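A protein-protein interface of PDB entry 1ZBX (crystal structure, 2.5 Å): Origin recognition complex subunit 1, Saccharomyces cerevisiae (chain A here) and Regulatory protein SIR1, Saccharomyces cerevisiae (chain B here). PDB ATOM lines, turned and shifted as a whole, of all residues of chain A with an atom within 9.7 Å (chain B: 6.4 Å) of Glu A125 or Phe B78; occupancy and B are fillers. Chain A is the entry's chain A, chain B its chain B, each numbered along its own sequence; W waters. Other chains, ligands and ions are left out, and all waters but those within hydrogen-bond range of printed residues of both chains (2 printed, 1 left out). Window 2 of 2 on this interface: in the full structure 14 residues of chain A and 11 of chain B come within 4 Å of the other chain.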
ATOM      1  N   TRP A  93      -9.735   3.423  37.857  1.00  0.00           N
ATOM      2  CA  TRP A  93      -9.659   4.795  37.364  1.00  0.00           C
ATOM      3  C   TRP A  93     -10.977   5.430  36.896  1.00  0.00           C
ATOM      4  O   TRP A  93     -11.318   6.536  37.321  1.00  0.00           O
ATOM      5  CB  TRP A  93      -8.621   4.893  36.241  1.00  0.00           C
ATOM      6  CG  TRP A  93      -8.981   4.092  35.058  1.00  0.00           C
ATOM      7  CD1 TRP A  93      -8.855   2.739  34.904  1.00  0.00           C
ATOM      8  CD2 TRP A  93      -9.604   4.574  33.872  1.00  0.00           C
ATOM      9  NE1 TRP A  93      -9.367   2.347  33.692  1.00  0.00           N
ATOM     10  CE2 TRP A  93      -9.834   3.454  33.034  1.00  0.00           C
ATOM     11  CE3 TRP A  93      -9.994   5.845  33.432  1.00  0.00           C
ATOM     12  CZ2 TRP A  93     -10.434   3.565  31.780  1.00  0.00           C
ATOM     13  CZ3 TRP A  93     -10.595   5.959  32.182  1.00  0.00           C
ATOM     14  CH2 TRP A  93     -10.809   4.820  31.368  1.00  0.00           C
ATOM     15  N   PHE A  94     -11.723   4.738  36.039  1.00  0.00           N
ATOM     16  CA  PHE A  94     -12.976   5.274  35.500  1.00  0.00           C
ATOM     17  C   PHE A  94     -14.135   5.499  36.485  1.00  0.00           C
ATOM     18  O   PHE A  94     -15.197   5.972  36.085  1.00  0.00           O
ATOM     19  CB  PHE A  94     -13.455   4.388  34.350  1.00  0.00           C
ATOM     20  CG  PHE A  94     -13.951   3.039  34.789  1.00  0.00           C
ATOM     21  CD1 PHE A  94     -15.266   2.869  35.210  1.00  0.00           C
ATOM     22  CD2 PHE A  94     -13.101   1.940  34.780  1.00  0.00           C
ATOM     23  CE1 PHE A  94     -15.727   1.620  35.612  1.00  0.00           C
ATOM     24  CE2 PHE A  94     -13.546   0.690  35.178  1.00  0.00           C
ATOM     25  CZ  PHE A  94     -14.859   0.521  35.595  1.00  0.00           C
ATOM     26  N   PRO A  98     -14.069  12.808  37.983  1.00  0.00           N
ATOM     27  CA  PRO A  98     -13.120  13.617  37.215  1.00  0.00           C
ATOM     28  C   PRO A  98     -12.961  15.050  37.692  1.00  0.00           C
ATOM     29  O   PRO A  98     -11.854  15.579  37.692  1.00  0.00           O
ATOM     30  CB  PRO A  98     -13.663  13.527  35.794  1.00  0.00           C
ATOM     31  CG  PRO A  98     -15.104  13.558  36.033  1.00  0.00           C
ATOM     32  CD  PRO A  98     -15.292  12.583  37.203  1.00  0.00           C
ATOM     33  N   ASN A 117     -16.765  16.945  29.179  1.00  0.00           N
ATOM     34  CA  ASN A 117     -16.064  15.965  28.343  1.00  0.00           C
ATOM     35  C   ASN A 117     -14.551  16.176  28.357  1.00  0.00           C
ATOM     36  O   ASN A 117     -13.777  15.224  28.260  1.00  0.00           O
ATOM     37  CB  ASN A 117     -16.604  16.010  26.899  1.00  0.00           C
ATOM     38  CG  ASN A 117     -16.446  17.389  26.242  1.00  0.00           C
ATOM     39  OD1 ASN A 117     -16.122  18.381  26.900  1.00  0.00           O
ATOM     40  ND2 ASN A 117     -16.694  17.450  24.939  1.00  0.00           N
ATOM     41  N   TYR A 118     -14.140  17.430  28.502  1.00  0.00           N
ATOM     42  CA  TYR A 118     -12.728  17.783  28.530  1.00  0.00           C
ATOM     43  C   TYR A 118     -12.019  17.207  29.762  1.00  0.00           C
ATOM     44  O   TYR A 118     -10.876  16.759  29.674  1.00  0.00           O
ATOM     45  CB  TYR A 118     -12.579  19.307  28.513  1.00  0.00           C
ATOM     46  CG  TYR A 118     -11.190  19.781  28.855  1.00  0.00           C
ATOM     47  CD1 TYR A 118     -10.243  20.010  27.856  1.00  0.00           C
ATOM     48  CD2 TYR A 118     -10.805  19.953  30.187  1.00  0.00           C
ATOM     49  CE1 TYR A 118      -8.947  20.398  28.177  1.00  0.00           C
ATOM     50  CE2 TYR A 118      -9.517  20.336  30.516  1.00  0.00           C
ATOM     51  CZ  TYR A 118      -8.593  20.558  29.510  1.00  0.00           C
ATOM     52  OH  TYR A 118      -7.314  20.937  29.840  1.00  0.00           O
ATOM     53  N   TYR A 119     -12.696  17.235  30.906  1.00  0.00           N
ATOM     54  CA  TYR A 119     -12.112  16.721  32.130  1.00  0.00           C
ATOM     55  C   TYR A 119     -12.145  15.214  32.108  1.00  0.00           C
ATOM     56  O   TYR A 119     -11.306  14.562  32.712  1.00  0.00           O
ATOM     57  CB  TYR A 119     -12.852  17.276  33.358  1.00  0.00           C
ATOM     58  CG  TYR A 119     -12.736  18.784  33.468  1.00  0.00           C
ATOM     59  CD1 TYR A 119     -13.778  19.618  33.046  1.00  0.00           C
ATOM     60  CD2 TYR A 119     -11.546  19.378  33.881  1.00  0.00           C
ATOM     61  CE1 TYR A 119     -13.632  20.997  33.023  1.00  0.00           C
ATOM     62  CE2 TYR A 119     -11.390  20.759  33.860  1.00  0.00           C
ATOM     63  CZ  TYR A 119     -12.435  21.565  33.425  1.00  0.00           C
ATOM     64  OH  TYR A 119     -12.262  22.930  33.359  1.00  0.00           O
ATOM     65  N   ASN A 120     -13.117  14.657  31.402  1.00  0.00           N
ATOM     66  CA  ASN A 120     -13.203  13.215  31.299  1.00  0.00           C
ATOM     67  C   ASN A 120     -11.970  12.727  30.535  1.00  0.00           C
ATOM     68  O   ASN A 120     -11.335  11.738  30.917  1.00  0.00           O
ATOM     69  CB  ASN A 120     -14.467  12.797  30.541  1.00  0.00           C
ATOM     70  CG  ASN A 120     -15.702  12.813  31.404  1.00  0.00           C
ATOM     71  OD1 ASN A 120     -15.638  12.514  32.596  1.00  0.00           O
ATOM     72  ND2 ASN A 120     -16.848  13.137  30.804  1.00  0.00           N
ATOM     73  N   LYS A 121     -11.643  13.442  29.460  1.00  0.00           N
ATOM     74  CA  LYS A 121     -10.521  13.120  28.593  1.00  0.00           C
ATOM     75  C   LYS A 121      -9.175  13.329  29.264  1.00  0.00           C
ATOM     76  O   LYS A 121      -8.276  12.492  29.159  1.00  0.00           O
ATOM     77  CB  LYS A 121     -10.577  13.978  27.332  1.00  0.00           C
ATOM     78  CG  LYS A 121      -9.403  13.750  26.393  1.00  0.00           C
ATOM     79  CD  LYS A 121      -9.329  14.826  25.339  1.00  0.00           C
ATOM     80  CE  LYS A 121      -8.310  14.478  24.283  1.00  0.00           C
ATOM     81  NZ  LYS A 121      -8.338  15.511  23.223  1.00  0.00           N
ATOM     82  N   LEU A 122      -9.034  14.470  29.926  1.00  0.00           N
ATOM     83  CA  LEU A 122      -7.804  14.798  30.617  1.00  0.00           C
ATOM     84  C   LEU A 122      -7.456  13.672  31.584  1.00  0.00           C
ATOM     85  O   LEU A 122      -6.381  13.079  31.504  1.00  0.00           O
ATOM     86  CB  LEU A 122      -7.974  16.102  31.394  1.00  0.00           C
ATOM     87  CG  LEU A 122      -6.694  16.622  32.044  1.00  0.00           C
ATOM     88  CD1 LEU A 122      -5.760  17.105  30.953  1.00  0.00           C
ATOM     89  CD2 LEU A 122      -7.004  17.753  33.018  1.00  0.00           C
ATOM     90  N   PHE A 123      -8.380  13.373  32.490  1.00  0.00           N
ATOM     91  CA  PHE A 123      -8.171  12.336  33.486  1.00  0.00           C
ATOM     92  C   PHE A 123      -7.888  10.967  32.878  1.00  0.00           C
ATOM     93  O   PHE A 123      -6.937  10.285  33.264  1.00  0.00           O
ATOM     94  CB  PHE A 123      -9.388  12.220  34.404  1.00  0.00           C
ATOM     95  CG  PHE A 123      -9.261  11.133  35.429  1.00  0.00           C
ATOM     96  CD1 PHE A 123      -8.406  11.279  36.516  1.00  0.00           C
ATOM     97  CD2 PHE A 123      -9.963   9.939  35.284  1.00  0.00           C
ATOM     98  CE1 PHE A 123      -8.255  10.252  37.446  1.00  0.00           C
ATOM     99  CE2 PHE A 123      -9.819   8.903  36.205  1.00  0.00           C
ATOM    100  CZ  PHE A 123      -8.965   9.058  37.287  1.00  0.00           C
ATOM    101  N   SER A 124      -8.723  10.570  31.931  1.00  0.00           N
ATOM    102  CA  SER A 124      -8.582   9.281  31.286  1.00  0.00           C
ATOM    103  C   SER A 124      -7.257   9.098  30.527  1.00  0.00           C
ATOM    104  O   SER A 124      -6.704   7.997  30.474  1.00  0.00           O
ATOM    105  CB  SER A 124      -9.766   9.074  30.345  1.00  0.00           C
ATOM    106  OG  SER A 124      -9.663   7.842  29.661  1.00  0.00           O
ATOM    107  N   GLU A 125      -6.744  10.178  29.950  1.00  0.00           N
ATOM    108  CA  GLU A 125      -5.507  10.100  29.186  1.00  0.00           C
ATOM    109  C   GLU A 125      -4.238  10.360  29.991  1.00  0.00           C
ATOM    110  O   GLU A 125      -3.139  10.316  29.433  1.00  0.00           O
ATOM    111  CB  GLU A 125      -5.558  11.062  27.990  1.00  0.00           C
ATOM    112  CG  GLU A 125      -6.758  10.848  27.078  1.00  0.00           C
ATOM    113  CD  GLU A 125      -6.601  11.492  25.705  1.00  0.00           C
ATOM    114  OE1 GLU A 125      -6.151  12.661  25.624  1.00  0.00           O
ATOM    115  OE2 GLU A 125      -6.946  10.823  24.705  1.00  0.00           O
ATOM    116  N   THR A 126      -4.372  10.628  31.289  1.00  0.00           N
ATOM    117  CA  THR A 126      -3.190  10.873  32.111  1.00  0.00           C
ATOM    118  C   THR A 126      -3.178  10.018  33.359  1.00  0.00           C
ATOM    119  O   THR A 126      -2.205  10.004  34.100  1.00  0.00           O
ATOM    120  CB  THR A 126      -3.079  12.354  32.541  1.00  0.00           C
ATOM    121  OG1 THR A 126      -4.216  12.708  33.333  1.00  0.00           O
ATOM    122  CG2 THR A 126      -2.997  13.267  31.315  1.00  0.00           C
ATOM    123  N   ALA A 127      -4.259   9.293  33.592  1.00  0.00           N
ATOM    124  CA  ALA A 127      -4.326   8.454  34.776  1.00  0.00           C
ATOM    125  C   ALA A 127      -3.645   7.117  34.554  1.00  0.00           C
ATOM    126  O   ALA A 127      -3.574   6.621  33.431  1.00  0.00           O
ATOM    127  CB  ALA A 127      -5.785   8.229  35.184  1.00  0.00           C
ATOM    128  N   ASN A 128      -3.122   6.541  35.627  1.00  0.00           N
ATOM    129  CA  ASN A 128      -2.506   5.236  35.529  1.00  0.00           C
ATOM    130  C   ASN A 128      -3.693   4.277  35.617  1.00  0.00           C
ATOM    131  O   ASN A 128      -4.227   4.041  36.704  1.00  0.00           O
ATOM    132  CB  ASN A 128      -1.555   4.994  36.695  1.00  0.00           C
ATOM    133  CG  ASN A 128      -1.157   3.537  36.818  1.00  0.00           C
ATOM    134  OD1 ASN A 128      -1.646   2.678  36.064  1.00  0.00           O
ATOM    135  ND2 ASN A 128      -0.277   3.239  37.770  1.00  0.00           N
ATOM    136  N   LYS A 129      -4.112   3.738  34.476  1.00  0.00           N
ATOM    137  CA  LYS A 129      -5.253   2.838  34.444  1.00  0.00           C
ATOM    138  C   LYS A 129      -5.098   1.564  35.255  1.00  0.00           C
ATOM    139  O   LYS A 129      -6.003   0.736  35.283  1.00  0.00           O
ATOM    140  CB  LYS A 129      -5.626   2.522  33.000  1.00  0.00           C
ATOM    141  CG  LYS A 129      -6.319   3.690  32.353  1.00  0.00           C
ATOM    142  CD  LYS A 129      -6.447   3.564  30.857  1.00  0.00           C
ATOM    143  CE  LYS A 129      -7.161   4.788  30.309  1.00  0.00           C
ATOM    144  NZ  LYS A 129      -7.155   4.816  28.825  1.00  0.00           N
ATOM    145  N   GLU B   8     -14.615  12.682  17.649  1.00  0.00           N
ATOM    146  CA  GLU B   8     -14.256  12.008  18.895  1.00  0.00           C
ATOM    147  C   GLU B   8     -14.724  12.760  20.145  1.00  0.00           C
ATOM    148  O   GLU B   8     -14.830  13.986  20.136  1.00  0.00           O
ATOM    149  CB  GLU B   8     -12.739  11.802  18.909  1.00  0.00           C
ATOM    150  CG  GLU B   8     -12.071  11.954  20.254  1.00  0.00           C
ATOM    151  CD  GLU B   8     -10.568  11.783  20.154  1.00  0.00           C
ATOM    152  OE1 GLU B   8      -9.954  12.422  19.272  1.00  0.00           O
ATOM    153  OE2 GLU B   8     -10.003  11.013  20.955  1.00  0.00           O
ATOM    154  N   TYR B  10     -15.321  12.044  24.813  1.00  0.00           N
ATOM    155  CA  TYR B  10     -15.477  11.207  26.001  1.00  0.00           C
ATOM    156  C   TYR B  10     -16.840  11.383  26.631  1.00  0.00           C
ATOM    157  O   TYR B  10     -17.070  12.338  27.360  1.00  0.00           O
ATOM    158  CB  TYR B  10     -14.419  11.535  27.053  1.00  0.00           C
ATOM    159  CG  TYR B  10     -13.073  10.914  26.793  1.00  0.00           C
ATOM    160  CD1 TYR B  10     -12.217  11.441  25.838  1.00  0.00           C
ATOM    161  CD2 TYR B  10     -12.656   9.793  27.504  1.00  0.00           C
ATOM    162  CE1 TYR B  10     -10.972  10.871  25.592  1.00  0.00           C
ATOM    163  CE2 TYR B  10     -11.418   9.212  27.270  1.00  0.00           C
ATOM    164  CZ  TYR B  10     -10.576   9.755  26.312  1.00  0.00           C
ATOM    165  OH  TYR B  10      -9.338   9.191  26.068  1.00  0.00           O
ATOM    166  N   LEU B  16     -15.684   6.231  25.372  1.00  0.00           N
ATOM    167  CA  LEU B  16     -15.153   7.164  24.385  1.00  0.00           C
ATOM    168  C   LEU B  16     -15.766   6.893  23.011  1.00  0.00           C
ATOM    169  O   LEU B  16     -15.760   5.759  22.543  1.00  0.00           O
ATOM    170  CB  LEU B  16     -13.636   6.977  24.319  1.00  0.00           C
ATOM    171  CG  LEU B  16     -12.815   7.601  23.204  1.00  0.00           C
ATOM    172  CD1 LEU B  16     -12.925   9.098  23.276  1.00  0.00           C
ATOM    173  CD2 LEU B  16     -11.377   7.176  23.351  1.00  0.00           C
ATOM    174  N   ILE B  23     -16.304   3.185  22.402  1.00  0.00           N
ATOM    175  CA  ILE B  23     -15.215   2.408  22.965  1.00  0.00           C
ATOM    176  C   ILE B  23     -15.227   2.332  24.484  1.00  0.00           C
ATOM    177  O   ILE B  23     -15.163   3.344  25.175  1.00  0.00           O
ATOM    178  CB  ILE B  23     -13.872   2.955  22.476  1.00  0.00           C
ATOM    179  CG1 ILE B  23     -13.817   2.834  20.957  1.00  0.00           C
ATOM    180  CG2 ILE B  23     -12.726   2.187  23.107  1.00  0.00           C
ATOM    181  CD1 ILE B  23     -12.602   3.486  20.330  1.00  0.00           C
ATOM    182  N   ASP B  24     -15.325   1.107  24.987  1.00  0.00           N
ATOM    183  CA  ASP B  24     -15.335   0.823  26.411  1.00  0.00           C
ATOM    184  C   ASP B  24     -13.874   0.748  26.863  1.00  0.00           C
ATOM    185  O   ASP B  24     -13.218  -0.284  26.718  1.00  0.00           O
ATOM    186  CB  ASP B  24     -16.026  -0.518  26.641  1.00  0.00           C
ATOM    187  CG  ASP B  24     -16.121  -0.895  28.097  1.00  0.00           C
ATOM    188  OD1 ASP B  24     -15.217  -0.515  28.879  1.00  0.00           O
ATOM    189  OD2 ASP B  24     -17.099  -1.594  28.446  1.00  0.00           O
ATOM    190  N   LEU B  25     -13.369   1.848  27.406  1.00  0.00           N
ATOM    191  CA  LEU B  25     -11.984   1.902  27.852  1.00  0.00           C
ATOM    192  C   LEU B  25     -11.670   0.966  29.012  1.00  0.00           C
ATOM    193  O   LEU B  25     -10.520   0.606  29.210  1.00  0.00           O
ATOM    194  CB  LEU B  25     -11.614   3.342  28.220  1.00  0.00           C
ATOM    195  CG  LEU B  25     -11.600   4.304  27.029  1.00  0.00           C
ATOM    196  CD1 LEU B  25     -11.513   5.740  27.513  1.00  0.00           C
ATOM    197  CD2 LEU B  25     -10.430   3.952  26.112  1.00  0.00           C
ATOM    198  N   GLU B  27     -12.614  -2.059  29.206  1.00  0.00           N
ATOM    199  CA  GLU B  27     -12.405  -3.367  28.602  1.00  0.00           C
ATOM    200  C   GLU B  27     -11.450  -3.321  27.413  1.00  0.00           C
ATOM    201  O   GLU B  27     -11.029  -4.363  26.910  1.00  0.00           O
ATOM    202  CB  GLU B  27     -13.757  -3.945  28.162  1.00  0.00           C
ATOM    203  CG  GLU B  27     -14.551  -4.566  29.295  1.00  0.00           C
ATOM    204  CD  GLU B  27     -13.850  -5.785  29.848  1.00  0.00           C
ATOM    205  OE1 GLU B  27     -13.695  -6.756  29.079  1.00  0.00           O
ATOM    206  OE2 GLU B  27     -13.445  -5.776  31.031  1.00  0.00           O
ATOM    207  N   GLU B  28     -11.112  -2.109  26.976  1.00  0.00           N
ATOM    208  CA  GLU B  28     -10.221  -1.893  25.837  1.00  0.00           C
ATOM    209  C   GLU B  28     -10.773  -2.523  24.551  1.00  0.00           C
ATOM    210  O   GLU B  28     -10.043  -3.149  23.779  1.00  0.00           O
ATOM    211  CB  GLU B  28      -8.820  -2.444  26.140  1.00  0.00           C
ATOM    212  CG  GLU B  28      -8.174  -1.833  27.382  1.00  0.00           C
ATOM    213  CD  GLU B  28      -6.695  -2.178  27.509  1.00  0.00           C
ATOM    214  OE1 GLU B  28      -5.864  -1.545  26.821  1.00  0.00           O
ATOM    215  OE2 GLU B  28      -6.364  -3.092  28.294  1.00  0.00           O
ATOM    216  N   LYS B  29     -12.067  -2.340  24.316  1.00  0.00           N
ATOM    217  CA  LYS B  29     -12.698  -2.901  23.134  1.00  0.00           C
ATOM    218  C   LYS B  29     -13.964  -2.146  22.761  1.00  0.00           C
ATOM    219  O   LYS B  29     -14.515  -1.404  23.564  1.00  0.00           O
ATOM    220  CB  LYS B  29     -13.050  -4.368  23.377  1.00  0.00           C
ATOM    221  CG  LYS B  29     -14.230  -4.549  24.303  1.00  0.00           C
ATOM    222  CD  LYS B  29     -14.480  -6.002  24.627  1.00  0.00           C
ATOM    223  CE  LYS B  29     -15.742  -6.139  25.461  1.00  0.00           C
ATOM    224  NZ  LYS B  29     -15.794  -7.406  26.241  1.00  0.00           N
ATOM    225  N   LYS B  73      -7.533   5.832  13.475  1.00  0.00           N
ATOM    226  CA  LYS B  73      -6.359   5.876  14.332  1.00  0.00           C
ATOM    227  C   LYS B  73      -6.710   5.774  15.811  1.00  0.00           C
ATOM    228  O   LYS B  73      -5.958   5.183  16.592  1.00  0.00           O
ATOM    229  CB  LYS B  73      -5.575   7.170  14.080  1.00  0.00           C
ATOM    230  CG  LYS B  73      -5.654   7.682  12.641  1.00  0.00           C
ATOM    231  CD  LYS B  73      -5.253   6.613  11.624  1.00  0.00           C
ATOM    232  CE  LYS B  73      -5.673   7.007  10.208  1.00  0.00           C
ATOM    233  NZ  LYS B  73      -5.508   5.879   9.240  1.00  0.00           N
ATOM    234  N   THR B  74      -7.857   6.336  16.190  1.00  0.00           N
ATOM    235  CA  THR B  74      -8.280   6.328  17.587  1.00  0.00           C
ATOM    236  C   THR B  74      -8.694   4.944  18.089  1.00  0.00           C
ATOM    237  O   THR B  74      -8.261   4.516  19.165  1.00  0.00           O
ATOM    238  CB  THR B  74      -9.450   7.327  17.835  1.00  0.00           C
ATOM    239  OG1 THR B  74      -9.122   8.604  17.277  1.00  0.00           O
ATOM    240  CG2 THR B  74      -9.691   7.516  19.333  1.00  0.00           C
ATOM    241  N   LEU B  75      -9.531   4.251  17.316  1.00  0.00           N
ATOM    242  CA  LEU B  75      -9.999   2.919  17.701  1.00  0.00           C
ATOM    243  C   LEU B  75      -8.840   1.969  17.982  1.00  0.00           C
ATOM    244  O   LEU B  75      -8.803   1.328  19.032  1.00  0.00           O
ATOM    245  CB  LEU B  75     -10.887   2.319  16.604  1.00  0.00           C
ATOM    246  CG  LEU B  75     -11.434   0.901  16.817  1.00  0.00           C
ATOM    247  CD1 LEU B  75     -12.554   0.916  17.826  1.00  0.00           C
ATOM    248  CD2 LEU B  75     -11.962   0.364  15.508  1.00  0.00           C
ATOM    249  N   PHE B  76      -7.891   1.882  17.054  1.00  0.00           N
ATOM    250  CA  PHE B  76      -6.748   0.990  17.228  1.00  0.00           C
ATOM    251  C   PHE B  76      -5.769   1.469  18.295  1.00  0.00           C
ATOM    252  O   PHE B  76      -4.898   0.723  18.745  1.00  0.00           O
ATOM    253  CB  PHE B  76      -6.019   0.793  15.898  1.00  0.00           C
ATOM    254  CG  PHE B  76      -6.864   0.144  14.850  1.00  0.00           C
ATOM    255  CD1 PHE B  76      -7.418   0.895  13.824  1.00  0.00           C
ATOM    256  CD2 PHE B  76      -7.162  -1.209  14.929  1.00  0.00           C
ATOM    257  CE1 PHE B  76      -8.261   0.310  12.894  1.00  0.00           C
ATOM    258  CE2 PHE B  76      -8.006  -1.808  14.006  1.00  0.00           C
ATOM    259  CZ  PHE B  76      -8.558  -1.048  12.987  1.00  0.00           C
ATOM    260  N   LYS B  77      -5.918   2.716  18.708  1.00  0.00           N
ATOM    261  CA  LYS B  77      -5.042   3.239  19.733  1.00  0.00           C
ATOM    262  C   LYS B  77      -5.483   2.734  21.099  1.00  0.00           C
ATOM    263  O   LYS B  77      -4.650   2.435  21.942  1.00  0.00           O
ATOM    264  CB  LYS B  77      -5.043   4.769  19.726  1.00  0.00           C
ATOM    265  CG  LYS B  77      -4.120   5.352  20.778  1.00  0.00           C
ATOM    266  CD  LYS B  77      -4.175   6.862  20.838  1.00  0.00           C
ATOM    267  CE  LYS B  77      -3.320   7.373  21.993  1.00  0.00           C
ATOM    268  NZ  LYS B  77      -3.452   8.846  22.204  1.00  0.00           N
ATOM    269  N   PHE B  78      -6.790   2.614  21.310  1.00  0.00           N
ATOM    270  CA  PHE B  78      -7.292   2.170  22.601  1.00  0.00           C
ATOM    271  C   PHE B  78      -7.807   0.744  22.730  1.00  0.00           C
ATOM    272  O   PHE B  78      -8.057   0.295  23.843  1.00  0.00           O
ATOM    273  CB  PHE B  78      -8.379   3.126  23.090  1.00  0.00           C
ATOM    274  CG  PHE B  78      -7.884   4.510  23.352  1.00  0.00           C
ATOM    275  CD1 PHE B  78      -8.095   5.523  22.426  1.00  0.00           C
ATOM    276  CD2 PHE B  78      -7.158   4.795  24.504  1.00  0.00           C
ATOM    277  CE1 PHE B  78      -7.585   6.810  22.641  1.00  0.00           C
ATOM    278  CE2 PHE B  78      -6.646   6.071  24.729  1.00  0.00           C
ATOM    279  CZ  PHE B  78      -6.860   7.081  23.793  1.00  0.00           C
ATOM    280  N   CYS B  79      -7.955   0.021  21.623  1.00  0.00           N
ATOM    281  CA  CYS B  79      -8.478  -1.347  21.691  1.00  0.00           C
ATOM    282  C   CYS B  79      -7.467  -2.493  21.655  1.00  0.00           C
ATOM    283  O   CYS B  79      -6.519  -2.472  20.880  1.00  0.00           O
ATOM    284  CB  CYS B  79      -9.502  -1.565  20.577  1.00  0.00           C
ATOM    285  SG  CYS B  79     -10.965  -0.529  20.706  1.00  0.00           S
ATOM    286  N   LYS B  80      -7.682  -3.497  22.500  1.00  0.00           N
ATOM    287  CA  LYS B  80      -6.809  -4.666  22.532  1.00  0.00           C
ATOM    288  C   LYS B  80      -6.836  -5.252  21.137  1.00  0.00           C
ATOM    289  O   LYS B  80      -7.838  -5.140  20.436  1.00  0.00           O
ATOM    290  CB  LYS B  80      -7.341  -5.751  23.476  1.00  0.00           C
ATOM    291  CG  LYS B  80      -7.209  -5.487  24.958  1.00  0.00           C
ATOM    292  CD  LYS B  80      -7.904  -6.600  25.750  1.00  0.00           C
ATOM    293  CE  LYS B  80      -7.852  -6.341  27.252  1.00  0.00           C
ATOM    294  NZ  LYS B  80      -8.745  -7.266  28.004  1.00  0.00           N
HETATM  295  O   HOH W   1     -14.141  14.759  24.876  1.00  0.00           O
HETATM  296  O   HOH W   2      -8.411   7.338  27.509  1.00  0.00           O
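Of the 16 printed residues of chain A, 6 touch a printed residue of chain B. Hydrophobic or aromatic side chains of chain A that line the printed part of chain B: Trp A93.
Water W2 lies within hydrogen-bond range of OH of Tyr B10 (2.5 Å), OG of Ser A124 (2.5 Å) and NZ of Lys A129 (3.1 Å). Water W1 lies within hydrogen-bond range of the backbone NH (N) of Tyr B10 (3.0 Å) and the backbone carbonyl oxygen (O) of Asn A117 (3.4 Å).
The side-chain carboxylate of Glu A125 lies within hydrogen-bond range of the side-chain hydroxyl of Tyr B10 (3.2 Å).
Leu B25 touches Trp A93 (CB to CH2, 3.6 Å). CB of Asn A117 touches O of Tyr B10, at 3.7 Å. Asn A120 touches Tyr B10 (ND2 to O, 3.5 Å). CB of Lys A121 touches CD1 of Tyr B10 (3.4 Å). CE2 of Tyr B10 touches OG of Ser A124 (3.3 Å). CD1 of Leu B25 touches OG of Ser A124, at 3.5 Å. Phe B78 touches Glu A125 (CZ to OE2, 3.9 Å).
Of the printed residues of chain B, Asn A117 touches Tyr B10 (3.7 Å). Printed residues of chain B within 4 Å of Asn A120: Tyr B10. Leu A122 touches none of the printed residues of chain B. Of the printed residues of chain B, Glu A125 touches Tyr B10 (3.2 Å) and Phe B78 (3.9 Å). Of the printed residues of chain A, Tyr B10 touches Asn A117, Asn A120, Lys A121, Ser A124 and Glu A125. No residue of chain A comes within 4 Å of Lys B77. Phe B78 touches one residue of chain A. No residue of chain A comes within 4 Å of Cys B79. Lys B80 touches none of the printed residues of chain A. The nearest residue of chain B that does not touch Glu A125 is Lys B77 (4.7 Å). The nearest residue of chain A that does not touch Phe B78 is Lys A129 (4.3 Å).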
